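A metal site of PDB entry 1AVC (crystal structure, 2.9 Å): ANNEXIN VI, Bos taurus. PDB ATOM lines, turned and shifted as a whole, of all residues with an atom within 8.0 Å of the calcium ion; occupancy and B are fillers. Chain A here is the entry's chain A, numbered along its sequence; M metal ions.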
ATOM      1  N   TYR A 609      32.501   8.915 -10.686  1.00  0.00           N
ATOM      2  CA  TYR A 609      31.284   9.546 -11.190  1.00  0.00           C
ATOM      3  C   TYR A 609      31.356   9.723 -12.699  1.00  0.00           C
ATOM      4  O   TYR A 609      30.402   9.420 -13.414  1.00  0.00           O
ATOM      5  CB  TYR A 609      31.087  10.916 -10.531  1.00  0.00           C
ATOM      6  CG  TYR A 609      29.812  11.607 -10.937  1.00  0.00           C
ATOM      7  CD1 TYR A 609      28.598  11.299 -10.326  1.00  0.00           C
ATOM      8  CD2 TYR A 609      29.809  12.569 -11.949  1.00  0.00           C
ATOM      9  CE1 TYR A 609      27.415  11.930 -10.698  1.00  0.00           C
ATOM     10  CE2 TYR A 609      28.633  13.208 -12.341  1.00  0.00           C
ATOM     11  CZ  TYR A 609      27.440  12.886 -11.713  1.00  0.00           C
ATOM     12  OH  TYR A 609      26.271  13.515 -12.086  1.00  0.00           O
ATOM     13  N   LYS A 610      32.500  10.191 -13.176  1.00  0.00           N
ATOM     14  CA  LYS A 610      32.705  10.413 -14.606  1.00  0.00           C
ATOM     15  C   LYS A 610      32.540   9.121 -15.394  1.00  0.00           C
ATOM     16  O   LYS A 610      31.888   9.089 -16.434  1.00  0.00           O
ATOM     17  CB  LYS A 610      34.104  10.984 -14.848  1.00  0.00           C
ATOM     18  CG  LYS A 610      34.126  12.483 -15.110  1.00  0.00           C
ATOM     19  CD  LYS A 610      34.799  13.227 -13.970  1.00  0.00           C
ATOM     20  CE  LYS A 610      35.546  14.457 -14.481  1.00  0.00           C
ATOM     21  NZ  LYS A 610      36.094  15.274 -13.361  1.00  0.00           N
ATOM     22  N   SER A 611      33.133   8.040 -14.894  1.00  0.00           N
ATOM     23  CA  SER A 611      33.061   6.740 -15.541  1.00  0.00           C
ATOM     24  C   SER A 611      31.621   6.298 -15.798  1.00  0.00           C
ATOM     25  O   SER A 611      31.339   5.613 -16.779  1.00  0.00           O
ATOM     26  CB  SER A 611      33.774   5.681 -14.700  1.00  0.00           C
ATOM     27  OG  SER A 611      33.083   5.433 -13.499  1.00  0.00           O
ATOM     28  N   MET A 612      30.721   6.703 -14.921  1.00  0.00           N
ATOM     29  CA  MET A 612      29.305   6.356 -15.051  1.00  0.00           C
ATOM     30  C   MET A 612      28.488   7.545 -15.546  1.00  0.00           C
ATOM     31  O   MET A 612      27.254   7.474 -15.641  1.00  0.00           O
ATOM     32  CB  MET A 612      28.755   5.866 -13.712  1.00  0.00           C
ATOM     33  CG  MET A 612      29.458   4.632 -13.181  1.00  0.00           C
ATOM     34  SD  MET A 612      28.773   4.072 -11.607  1.00  0.00           S
ATOM     35  CE  MET A 612      29.359   5.349 -10.508  1.00  0.00           C
ATOM     36  N   LYS A 613      29.173   8.643 -15.851  1.00  0.00           N
ATOM     37  CA  LYS A 613      28.519   9.847 -16.341  1.00  0.00           C
ATOM     38  C   LYS A 613      28.346   9.774 -17.857  1.00  0.00           C
ATOM     39  O   LYS A 613      29.254   9.364 -18.573  1.00  0.00           O
ATOM     40  CB  LYS A 613      29.360  11.080 -15.970  1.00  0.00           C
ATOM     41  CG  LYS A 613      29.056  12.322 -16.790  1.00  0.00           C
ATOM     42  CD  LYS A 613      30.264  13.239 -16.875  1.00  0.00           C
ATOM     43  CE  LYS A 613      30.970  13.118 -18.210  1.00  0.00           C
ATOM     44  NZ  LYS A 613      31.038  11.697 -18.681  1.00  0.00           N
ATOM     45  N   GLY A 614      27.164  10.165 -18.320  1.00  0.00           N
ATOM     46  CA  GLY A 614      26.871  10.137 -19.745  1.00  0.00           C
ATOM     47  C   GLY A 614      26.072   8.896 -20.120  1.00  0.00           C
ATOM     48  O   GLY A 614      25.690   8.115 -19.253  1.00  0.00           O
ATOM     49  N   ALA A 615      25.810   8.731 -21.404  1.00  0.00           N
ATOM     50  CA  ALA A 615      25.040   7.585 -21.885  1.00  0.00           C
ATOM     51  C   ALA A 615      25.839   6.285 -21.765  1.00  0.00           C
ATOM     52  O   ALA A 615      25.287   5.243 -21.406  1.00  0.00           O
ATOM     53  CB  ALA A 615      24.633   7.799 -23.339  1.00  0.00           C
ATOM     54  N   GLY A 616      27.136   6.364 -22.054  1.00  0.00           N
ATOM     55  CA  GLY A 616      27.988   5.200 -21.967  1.00  0.00           C
ATOM     56  C   GLY A 616      28.553   4.975 -20.575  1.00  0.00           C
ATOM     57  O   GLY A 616      28.186   5.659 -19.637  1.00  0.00           O
ATOM     58  N   THR A 617      29.463   4.013 -20.446  1.00  0.00           N
ATOM     59  CA  THR A 617      30.082   3.710 -19.159  1.00  0.00           C
ATOM     60  C   THR A 617      31.493   3.200 -19.394  1.00  0.00           C
ATOM     61  O   THR A 617      31.724   2.450 -20.336  1.00  0.00           O
ATOM     62  CB  THR A 617      29.291   2.610 -18.412  1.00  0.00           C
ATOM     63  OG1 THR A 617      28.003   3.116 -18.033  1.00  0.00           O
ATOM     64  CG2 THR A 617      30.040   2.176 -17.155  1.00  0.00           C
ATOM     65  N   GLU A 618      32.425   3.620 -18.551  1.00  0.00           N
ATOM     66  CA  GLU A 618      33.799   3.164 -18.684  1.00  0.00           C
ATOM     67  C   GLU A 618      34.066   2.091 -17.641  1.00  0.00           C
ATOM     68  O   GLU A 618      34.643   2.362 -16.594  1.00  0.00           O
ATOM     69  CB  GLU A 618      34.784   4.316 -18.514  1.00  0.00           C
ATOM     70  CG  GLU A 618      36.234   3.887 -18.598  1.00  0.00           C
ATOM     71  CD  GLU A 618      37.194   5.049 -18.616  1.00  0.00           C
ATOM     72  OE1 GLU A 618      36.845   6.124 -18.093  1.00  0.00           O
ATOM     73  OE2 GLU A 618      38.306   4.882 -19.158  1.00  0.00           O
ATOM     74  N   GLU A 619      33.607   0.873 -17.927  1.00  0.00           N
ATOM     75  CA  GLU A 619      33.793  -0.247 -17.012  1.00  0.00           C
ATOM     76  C   GLU A 619      35.257  -0.436 -16.657  1.00  0.00           C
ATOM     77  O   GLU A 619      35.577  -0.987 -15.607  1.00  0.00           O
ATOM     78  CB  GLU A 619      33.236  -1.530 -17.627  1.00  0.00           C
ATOM     79  CG  GLU A 619      33.067  -1.473 -19.139  1.00  0.00           C
ATOM     80  CD  GLU A 619      31.784  -0.771 -19.563  1.00  0.00           C
ATOM     81  OE1 GLU A 619      30.776  -0.867 -18.838  1.00  0.00           O
ATOM     82  OE2 GLU A 619      31.793  -0.124 -20.630  1.00  0.00           O
ATOM     83  N   ALA A 652      24.422   4.460  -8.094  1.00  0.00           N
ATOM     84  CA  ALA A 652      25.190   4.951  -9.228  1.00  0.00           C
ATOM     85  C   ALA A 652      25.561   3.794 -10.136  1.00  0.00           C
ATOM     86  O   ALA A 652      25.358   3.850 -11.346  1.00  0.00           O
ATOM     87  CB  ALA A 652      26.447   5.661  -8.740  1.00  0.00           C
ATOM     88  N   GLY A 655      22.541   1.650 -11.603  1.00  0.00           N
ATOM     89  CA  GLY A 655      21.897   2.202 -12.778  1.00  0.00           C
ATOM     90  C   GLY A 655      22.669   2.066 -14.067  1.00  0.00           C
ATOM     91  O   GLY A 655      22.084   1.992 -15.150  1.00  0.00           O
ATOM     92  N   ASP A 656      23.983   2.023 -13.961  1.00  0.00           N
ATOM     93  CA  ASP A 656      24.830   1.914 -15.147  1.00  0.00           C
ATOM     94  C   ASP A 656      25.142   0.484 -15.556  1.00  0.00           C
ATOM     95  O   ASP A 656      24.892   0.084 -16.697  1.00  0.00           O
ATOM     96  CB  ASP A 656      26.123   2.673 -14.893  1.00  0.00           C
ATOM     97  CG  ASP A 656      26.118   4.045 -15.514  1.00  0.00           C
ATOM     98  OD1 ASP A 656      25.102   4.769 -15.375  1.00  0.00           O
ATOM     99  OD2 ASP A 656      27.132   4.408 -16.136  1.00  0.00           O
ATOM    100  N   THR A 657      25.733  -0.276 -14.642  1.00  0.00           N
ATOM    101  CA  THR A 657      26.072  -1.664 -14.932  1.00  0.00           C
ATOM    102  C   THR A 657      24.872  -2.576 -14.714  1.00  0.00           C
ATOM    103  O   THR A 657      23.860  -2.163 -14.149  1.00  0.00           O
ATOM    104  CB  THR A 657      27.232  -2.172 -14.040  1.00  0.00           C
ATOM    105  OG1 THR A 657      26.793  -2.261 -12.679  1.00  0.00           O
ATOM    106  CG2 THR A 657      28.425  -1.223 -14.134  1.00  0.00           C
HETATM  107 CA    CA M   1      26.396   5.663 -18.196  1.00  0.00          CA
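The side-chain hydroxyl (OG1) of Thr 617 lies close to the side-chain carboxylate (OD2) of Asp 656, 2.5 Å away. The backbone carbonyl oxygen (O) of Thr 617 lies close to the side-chain carboxylate (OE2) of Glu 619.
Residues that only touch the calcium ion: Met 612 (3.2 Å) and Ala 615 (3.4 Å). Of the 15 residues printed, 6 come within 4 Å of the calcium ion.
The calcium ion is bound by the backbone carbonyl oxygen (O) of Gly 616 (2.3 Å), the side-chain carboxylate (OD2) of Asp 656 (2.5 Å) and the backbone carbonyl oxygen (O) of Gly 614 (2.8 Å). The calcium ion has three donor atoms within binding distance. Slightly farther from the calcium ion lies OG1 of Thr 617 (3.0 Å).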
